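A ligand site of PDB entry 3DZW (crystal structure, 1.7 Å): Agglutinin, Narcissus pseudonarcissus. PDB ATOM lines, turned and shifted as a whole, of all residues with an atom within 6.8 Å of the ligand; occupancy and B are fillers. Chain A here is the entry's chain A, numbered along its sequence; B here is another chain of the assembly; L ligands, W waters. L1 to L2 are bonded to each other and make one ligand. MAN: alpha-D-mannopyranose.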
ATOM      1  N   GLN A  89     -20.333 -10.697 -25.091  1.00  0.00           N
ATOM      2  CA  GLN A  89     -20.883  -9.349 -25.368  1.00  0.00           C
ATOM      3  C   GLN A  89     -21.936  -9.242 -26.475  1.00  0.00           C
ATOM      4  O   GLN A  89     -22.046 -10.100 -27.346  1.00  0.00           O
ATOM      5  CB  GLN A  89     -19.713  -8.385 -25.688  1.00  0.00           C
ATOM      6  CG  GLN A  89     -18.661  -8.317 -24.552  1.00  0.00           C
ATOM      7  CD  GLN A  89     -17.521  -7.327 -24.811  1.00  0.00           C
ATOM      8  OE1 GLN A  89     -16.733  -7.045 -23.907  1.00  0.00           O
ATOM      9  NE2 GLN A  89     -17.448  -6.797 -26.027  1.00  0.00           N
ATOM     10  N   ASP A  91     -21.858  -7.305 -28.914  1.00  0.00           N
ATOM     11  CA  ASP A  91     -21.193  -7.084 -30.228  1.00  0.00           C
ATOM     12  C   ASP A  91     -20.554  -8.383 -30.774  1.00  0.00           C
ATOM     13  O   ASP A  91     -19.827  -8.348 -31.746  1.00  0.00           O
ATOM     14  CB  ASP A  91     -20.144  -5.933 -30.164  1.00  0.00           C
ATOM     15  CG  ASP A  91     -18.896  -6.284 -29.317  1.00  0.00           C
ATOM     16  OD1 ASP A  91     -18.859  -7.335 -28.647  1.00  0.00           O
ATOM     17  OD2 ASP A  91     -17.948  -5.474 -29.339  1.00  0.00           O
ATOM     18  N   ARG A  92     -20.816  -9.519 -30.081  1.00  0.00           N
ATOM     19  CA  ARG A  92     -20.349 -10.887 -30.479  1.00  0.00           C
ATOM     20  C   ARG A  92     -18.886 -11.251 -30.026  1.00  0.00           C
ATOM     21  O   ARG A  92     -18.403 -12.340 -30.308  1.00  0.00           O
ATOM     22  CB  ARG A  92     -20.518 -11.126 -32.006  1.00  0.00           C
ATOM     23  CG  ARG A  92     -20.646 -12.625 -32.376  1.00  0.00           C
ATOM     24  CD  ARG A  92     -20.849 -12.874 -33.882  1.00  0.00           C
ATOM     25  NE  ARG A  92     -19.619 -12.677 -34.643  1.00  0.00           N
ATOM     26  CZ  ARG A  92     -19.486 -12.914 -35.954  1.00  0.00           C
ATOM     27  NH1 ARG A  92     -20.523 -13.368 -36.668  1.00  0.00           N
ATOM     28  NH2 ARG A  92     -18.327 -12.706 -36.548  1.00  0.00           N
ATOM     29  N   ASN A  93     -18.223 -10.350 -29.321  1.00  0.00           N
ATOM     30  CA  ASN A  93     -16.895 -10.620 -28.856  1.00  0.00           C
ATOM     31  C   ASN A  93     -17.003 -11.298 -27.486  1.00  0.00           C
ATOM     32  O   ASN A  93     -17.979 -11.077 -26.762  1.00  0.00           O
ATOM     33  CB  ASN A  93     -16.087  -9.310 -28.759  1.00  0.00           C
ATOM     34  CG  ASN A  93     -14.535  -9.508 -28.939  1.00  0.00           C
ATOM     35  OD1 ASN A  93     -14.049 -10.636 -29.130  1.00  0.00           O
ATOM     36  ND2 ASN A  93     -13.786  -8.396 -28.906  1.00  0.00           N
ATOM     37  N   VAL A  94     -16.024 -12.160 -27.156  1.00  0.00           N
ATOM     38  CA  VAL A  94     -15.945 -12.820 -25.843  1.00  0.00           C
ATOM     39  C   VAL A  94     -14.672 -12.222 -25.231  1.00  0.00           C
ATOM     40  O   VAL A  94     -13.574 -12.408 -25.777  1.00  0.00           O
ATOM     41  CB  VAL A  94     -15.884 -14.328 -25.939  1.00  0.00           C
ATOM     42  CG1 VAL A  94     -15.704 -14.939 -24.567  1.00  0.00           C
ATOM     43  CG2 VAL A  94     -17.143 -14.882 -26.624  1.00  0.00           C
ATOM     44  N   VAL A  95     -14.822 -11.506 -24.103  1.00  0.00           N
ATOM     45  CA  VAL A  95     -13.713 -10.779 -23.481  1.00  0.00           C
ATOM     46  C   VAL A  95     -13.539 -10.971 -21.970  1.00  0.00           C
ATOM     47  O   VAL A  95     -14.516 -11.038 -21.221  1.00  0.00           O
ATOM     48  CB  VAL A  95     -13.914  -9.231 -23.718  1.00  0.00           C
ATOM     49  CG1 VAL A  95     -12.689  -8.442 -23.278  1.00  0.00           C
ATOM     50  CG2 VAL A  95     -14.221  -8.946 -25.173  1.00  0.00           C
ATOM     51  N   TYR A  97     -12.192  -9.284 -18.529  1.00  0.00           N
ATOM     52  CA  TYR A  97     -11.886  -7.972 -17.918  1.00  0.00           C
ATOM     53  C   TYR A  97     -11.508  -8.143 -16.447  1.00  0.00           C
ATOM     54  O   TYR A  97     -12.037  -9.022 -15.774  1.00  0.00           O
ATOM     55  CB  TYR A  97     -13.077  -7.026 -17.956  1.00  0.00           C
ATOM     56  CG  TYR A  97     -13.581  -6.594 -19.319  1.00  0.00           C
ATOM     57  CD1 TYR A  97     -14.600  -7.281 -19.964  1.00  0.00           C
ATOM     58  CD2 TYR A  97     -13.072  -5.450 -19.936  1.00  0.00           C
ATOM     59  CE1 TYR A  97     -15.092  -6.872 -21.205  1.00  0.00           C
ATOM     60  CE2 TYR A  97     -13.549  -5.023 -21.172  1.00  0.00           C
ATOM     61  CZ  TYR A  97     -14.564  -5.738 -21.804  1.00  0.00           C
ATOM     62  OH  TYR A  97     -15.041  -5.311 -23.040  1.00  0.00           O
ATOM     63  N   TYR B   5     -20.944  -0.354 -21.225  1.00  0.00           N
ATOM     64  CA  TYR B   5     -19.581  -0.479 -21.803  1.00  0.00           C
ATOM     65  C   TYR B   5     -18.877   0.861 -21.903  1.00  0.00           C
ATOM     66  O   TYR B   5     -19.518   1.906 -22.015  1.00  0.00           O
ATOM     67  CB  TYR B   5     -19.647  -1.128 -23.196  1.00  0.00           C
ATOM     68  CG  TYR B   5     -20.108  -2.580 -23.199  1.00  0.00           C
ATOM     69  CD1 TYR B   5     -21.451  -2.908 -23.280  1.00  0.00           C
ATOM     70  CD2 TYR B   5     -19.174  -3.621 -23.124  1.00  0.00           C
ATOM     71  CE1 TYR B   5     -21.867  -4.259 -23.278  1.00  0.00           C
ATOM     72  CE2 TYR B   5     -19.584  -4.964 -23.114  1.00  0.00           C
ATOM     73  CZ  TYR B   5     -20.922  -5.269 -23.199  1.00  0.00           C
ATOM     74  OH  TYR B   5     -21.323  -6.594 -23.200  1.00  0.00           O
ATOM     75  N   SER B   6     -17.527   0.833 -21.846  1.00  0.00           N
ATOM     76  CA  SER B   6     -16.746   2.078 -21.983  1.00  0.00           C
ATOM     77  C   SER B   6     -17.056   2.690 -23.344  1.00  0.00           C
ATOM     78  O   SER B   6     -17.096   1.968 -24.370  1.00  0.00           O
ATOM     79  CB  SER B   6     -15.229   1.855 -21.767  1.00  0.00           C
ATOM     80  OG  SER B   6     -14.693   0.878 -22.636  1.00  0.00           O
ATOM     81  N   GLY B  82      -8.185   2.363 -22.451  1.00  0.00           N
ATOM     82  CA  GLY B  82      -8.485   0.976 -22.800  1.00  0.00           C
ATOM     83  C   GLY B  82      -9.973   0.671 -22.827  1.00  0.00           C
ATOM     84  O   GLY B  82     -10.792   1.567 -23.059  1.00  0.00           O
ATOM     85  N   ASN B  83     -10.311  -0.601 -22.594  1.00  0.00           N
ATOM     86  CA  ASN B  83     -11.696  -1.069 -22.602  1.00  0.00           C
ATOM     87  C   ASN B  83     -12.111  -1.525 -21.212  1.00  0.00           C
ATOM     88  O   ASN B  83     -11.438  -2.352 -20.589  1.00  0.00           O
ATOM     89  CB  ASN B  83     -11.860  -2.201 -23.610  1.00  0.00           C
ATOM     90  CG  ASN B  83     -11.657  -1.721 -25.074  1.00  0.00           C
ATOM     91  OD1 ASN B  83     -12.415  -0.908 -25.584  1.00  0.00           O
ATOM     92  ND2 ASN B  83     -10.650  -2.267 -25.728  1.00  0.00           N
ATOM     93  N   TYR B  84     -13.233  -0.976 -20.723  1.00  0.00           N
ATOM     94  CA  TYR B  84     -13.763  -1.278 -19.391  1.00  0.00           C
ATOM     95  C   TYR B  84     -15.248  -1.582 -19.432  1.00  0.00           C
ATOM     96  O   TYR B  84     -15.911  -1.318 -20.429  1.00  0.00           O
ATOM     97  CB  TYR B  84     -13.560  -0.066 -18.463  1.00  0.00           C
ATOM     98  CG  TYR B  84     -12.128   0.394 -18.274  1.00  0.00           C
ATOM     99  CD1 TYR B  84     -11.498   1.223 -19.206  1.00  0.00           C
ATOM    100  CD2 TYR B  84     -11.411   0.052 -17.129  1.00  0.00           C
ATOM    101  CE1 TYR B  84     -10.176   1.660 -19.019  1.00  0.00           C
ATOM    102  CE2 TYR B  84     -10.092   0.495 -16.934  1.00  0.00           C
ATOM    103  CZ  TYR B  84      -9.493   1.294 -17.883  1.00  0.00           C
ATOM    104  OH  TYR B  84      -8.193   1.731 -17.692  1.00  0.00           O
ATOM    105  N   VAL B  85     -15.770  -2.131 -18.316  1.00  0.00           N
ATOM    106  CA  VAL B  85     -17.193  -2.417 -18.177  1.00  0.00           C
ATOM    107  C   VAL B  85     -17.706  -2.099 -16.771  1.00  0.00           C
ATOM    108  O   VAL B  85     -17.008  -2.316 -15.799  1.00  0.00           O
ATOM    109  CB  VAL B  85     -17.562  -3.926 -18.492  1.00  0.00           C
ATOM    110  CG1 VAL B  85     -17.359  -4.246 -19.978  1.00  0.00           C
ATOM    111  CG2 VAL B  85     -16.769  -4.899 -17.592  1.00  0.00           C
ATOM    112  N   ALA B 100      -9.182  -4.773 -20.687  1.00  0.00           N
ATOM    113  CA  ALA B 100      -9.369  -6.094 -21.348  1.00  0.00           C
ATOM    114  C   ALA B 100      -8.037  -6.852 -21.367  1.00  0.00           C
ATOM    115  O   ALA B 100      -7.025  -6.323 -21.829  1.00  0.00           O
ATOM    116  CB  ALA B 100      -9.903  -5.919 -22.740  1.00  0.00           C
ATOM    117  N   TRP B 102      -7.845 -10.355 -22.516  1.00  0.00           N
ATOM    118  CA  TRP B 102      -7.870 -11.297 -23.625  1.00  0.00           C
ATOM    119  C   TRP B 102      -9.219 -11.244 -24.315  1.00  0.00           C
ATOM    120  O   TRP B 102     -10.198 -10.851 -23.699  1.00  0.00           O
ATOM    121  CB  TRP B 102      -7.586 -12.722 -23.094  1.00  0.00           C
ATOM    122  CG  TRP B 102      -7.795 -13.852 -24.096  1.00  0.00           C
ATOM    123  CD1 TRP B 102      -6.871 -14.377 -24.930  1.00  0.00           C
ATOM    124  CD2 TRP B 102      -9.019 -14.575 -24.327  1.00  0.00           C
ATOM    125  NE1 TRP B 102      -7.432 -15.380 -25.683  1.00  0.00           N
ATOM    126  CE2 TRP B 102      -8.746 -15.526 -25.338  1.00  0.00           C
ATOM    127  CE3 TRP B 102     -10.305 -14.508 -23.791  1.00  0.00           C
ATOM    128  CZ2 TRP B 102      -9.728 -16.407 -25.812  1.00  0.00           C
ATOM    129  CZ3 TRP B 102     -11.284 -15.395 -24.273  1.00  0.00           C
ATOM    130  CH2 TRP B 102     -10.977 -16.322 -25.274  1.00  0.00           C
ATOM    131  N   ALA B 103      -9.265 -11.627 -25.594  1.00  0.00           N
ATOM    132  CA  ALA B 103     -10.515 -11.640 -26.366  1.00  0.00           C
ATOM    133  C   ALA B 103     -10.445 -12.589 -27.566  1.00  0.00           C
ATOM    134  O   ALA B 103      -9.372 -12.841 -28.109  1.00  0.00           O
ATOM    135  CB  ALA B 103     -10.881 -10.240 -26.828  1.00  0.00           C
ATOM    136  N   GLY B 105     -11.752 -11.941 -30.448  1.00  0.00           N
ATOM    137  CA  GLY B 105     -11.608 -11.098 -31.652  1.00  0.00           C
ATOM    138  C   GLY B 105     -12.713 -11.333 -32.669  1.00  0.00           C
ATOM    139  O   GLY B 105     -12.515 -11.150 -33.880  1.00  0.00           O
ATOM    140  N   ASN B 107     -15.733  -9.688 -32.663  1.00  0.00           N
ATOM    141  CA  ASN B 107     -16.657  -8.550 -32.662  1.00  0.00           C
ATOM    142  C   ASN B 107     -17.094  -8.142 -34.058  1.00  0.00           C
ATOM    143  O   ASN B 107     -16.362  -8.327 -35.021  1.00  0.00           O
ATOM    144  CB  ASN B 107     -16.042  -7.317 -31.957  1.00  0.00           C
ATOM    145  CG  ASN B 107     -14.738  -6.854 -32.608  1.00  0.00           C
ATOM    146  OD1 ASN B 107     -13.841  -7.651 -32.873  1.00  0.00           O
ATOM    147  ND2 ASN B 107     -14.633  -5.544 -32.838  1.00  0.00           N
ATOM    148  N   ILE B 108     -18.302  -7.595 -34.150  1.00  0.00           N
ATOM    149  CA  ILE B 108     -18.844  -7.096 -35.421  1.00  0.00           C
ATOM    150  C   ILE B 108     -19.436  -5.712 -35.204  1.00  0.00           C
ATOM    151  O   ILE B 108     -19.721  -5.328 -34.060  1.00  0.00           O
ATOM    152  CB  ILE B 108     -19.896  -8.072 -36.040  1.00  0.00           C
ATOM    153  CG1 ILE B 108     -21.106  -8.241 -35.113  1.00  0.00           C
ATOM    154  CG2 ILE B 108     -19.280  -9.418 -36.320  1.00  0.00           C
ATOM    155  CD1 ILE B 108     -22.146  -9.210 -35.650  1.00  0.00           C
ATOM    156  N   HIS B 109     -19.600  -4.960 -36.287  1.00  0.00           N
ATOM    157  CA  HIS B 109     -20.167  -3.601 -36.205  1.00  0.00           C
ATOM    158  C   HIS B 109     -21.671  -3.623 -36.469  1.00  0.00           C
ATOM    159  O   HIS B 109     -22.323  -2.568 -36.540  1.00  0.00           O
ATOM    160  CB  HIS B 109     -19.468  -2.677 -37.189  1.00  0.00           C
ATOM    161  CG  HIS B 109     -18.023  -2.446 -36.866  1.00  0.00           C
ATOM    162  ND1 HIS B 109     -17.015  -3.256 -37.335  1.00  0.00           N
ATOM    163  CD2 HIS B 109     -17.427  -1.493 -36.111  1.00  0.00           C
ATOM    164  CE1 HIS B 109     -15.855  -2.808 -36.895  1.00  0.00           C
ATOM    165  NE2 HIS B 109     -16.070  -1.743 -36.152  1.00  0.00           N
ATOM    166  OXT HIS B 109     -22.280  -4.684 -36.623  1.00  0.00           O
HETATM  167  C1  MAN L   1      -9.445  -2.191 -30.630  1.00  0.00           C
HETATM  168  C2  MAN L   1     -10.544  -2.643 -29.564  1.00  0.00           C
HETATM  169  C3  MAN L   1     -11.846  -3.084 -30.240  1.00  0.00           C
HETATM  170  C4  MAN L   1     -12.249  -2.105 -31.332  1.00  0.00           C
HETATM  171  C5  MAN L   1     -11.178  -1.999 -32.421  1.00  0.00           C
HETATM  172  C6  MAN L   1     -11.610  -1.049 -33.543  1.00  0.00           C
HETATM  173  O1  MAN L   1      -8.231  -3.081 -30.771  1.00  0.00           O
HETATM  174  O2  MAN L   1     -10.794  -1.607 -28.672  1.00  0.00           O
HETATM  175  O3  MAN L   1     -12.905  -3.212 -29.281  1.00  0.00           O
HETATM  176  O4  MAN L   1     -13.461  -2.517 -31.923  1.00  0.00           O
HETATM  177  O5  MAN L   1      -9.964  -1.510 -31.894  1.00  0.00           O
HETATM  178  O6  MAN L   1     -11.644   0.275 -33.039  1.00  0.00           O
HETATM  179  C1  MAN L   2     -13.439  -4.554 -29.229  1.00  0.00           C
HETATM  180  C2  MAN L   2     -14.743  -4.537 -28.447  1.00  0.00           C
HETATM  181  C3  MAN L   2     -14.488  -4.212 -26.983  1.00  0.00           C
HETATM  182  C4  MAN L   2     -13.463  -5.168 -26.399  1.00  0.00           C
HETATM  183  C5  MAN L   2     -12.201  -5.192 -27.276  1.00  0.00           C
HETATM  184  C6  MAN L   2     -11.193  -6.214 -26.781  1.00  0.00           C
HETATM  185  O2  MAN L   2     -15.396  -5.802 -28.584  1.00  0.00           O
HETATM  186  O3  MAN L   2     -15.692  -4.299 -26.235  1.00  0.00           O
HETATM  187  O4  MAN L   2     -13.134  -4.773 -25.073  1.00  0.00           O
HETATM  188  O5  MAN L   2     -12.550  -5.480 -28.647  1.00  0.00           O
HETATM  189  O6  MAN L   2     -10.008  -6.147 -27.563  1.00  0.00           O
HETATM  190  O   HOH W   1     -13.720  -0.801 -28.529  1.00  0.00           O
HETATM  191  O   HOH W   2      -8.033  -4.216 -27.477  1.00  0.00           O
HETATM  192  O   HOH W   3     -10.518  -8.140 -29.921  1.00  0.00           O
HETATM  193  O   HOH W   4      -8.018  -8.186 -25.560  1.00  0.00           O
HETATM  194  O   HOH W   5     -11.046   1.100 -29.651  1.00  0.00           O
HETATM  195  O   HOH W   6     -15.888  -1.570 -31.623  1.00  0.00           O
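Hydrophobic or aromatic side chains that line the ligand: Tyr 97. Along chain A the residues within 4 Å of the ligand span positions 89 to 97. The nearest printed residue that does not touch the ligand is Ala 103 of chain B (4.04 Å).
Water W1 bridges O3 of MAN L1 (2.7 Å) and OD1 of Asn 83 of chain B (3.2 Å). Water W3 lies within hydrogen-bond range of an oxygen (O6) of MAN L2 and the side-chain amide nitrogen (ND2) of Asn 93.
OD2 of Asp 91 lies within hydrogen-bond range of O2 of MAN L2, 2.7 Å away. The side-chain hydroxyl of Tyr 97 is in hydrogen-bond range of an oxygen (O4) of MAN L2, at 2.8 Å. The side-chain amide nitrogen of Asn 83 of chain B lies within hydrogen-bond range of an oxygen (O2) of MAN L1 (3.0 Å). An oxygen (O3) of MAN L2 is in hydrogen-bond range of the side-chain amide nitrogen of Gln 89, 3.1 Å away. O2 of MAN L2 lies within hydrogen-bond range of ND2 of Asn 93, at 3.1 Å. An oxygen (O4) of MAN L1 is in hydrogen-bond range of the side-chain amide nitrogen (ND2) of Asn 107 of chain B, 3.4 Å away.
The side-chain carboxylate (OD1) of Asp 91 sits at hydrogen-bond distance from the side-chain amide nitrogen (NE2) of Gln 89 (3.0 Å). The backbone NH (N) of Asn 93 sits at hydrogen-bond distance from the side-chain carboxylate (OD1) of Asp 91 (3.2 Å). O of Asp 91 sits at hydrogen-bond distance from N of Ile 108 of chain B (2.9 Å). The side-chain hydroxyl (OH) of Tyr 97 is in hydrogen-bond range of the side-chain amide oxygen (OE1) of Gln 89 (2.6 Å). The backbone carbonyl oxygen of Asn 83 of chain B lies within hydrogen-bond range of the backbone NH of Ala 100 of chain B, at 3.3 Å. OD1 of Asn 93 sits at hydrogen-bond distance from N of Gly 105 of chain B.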
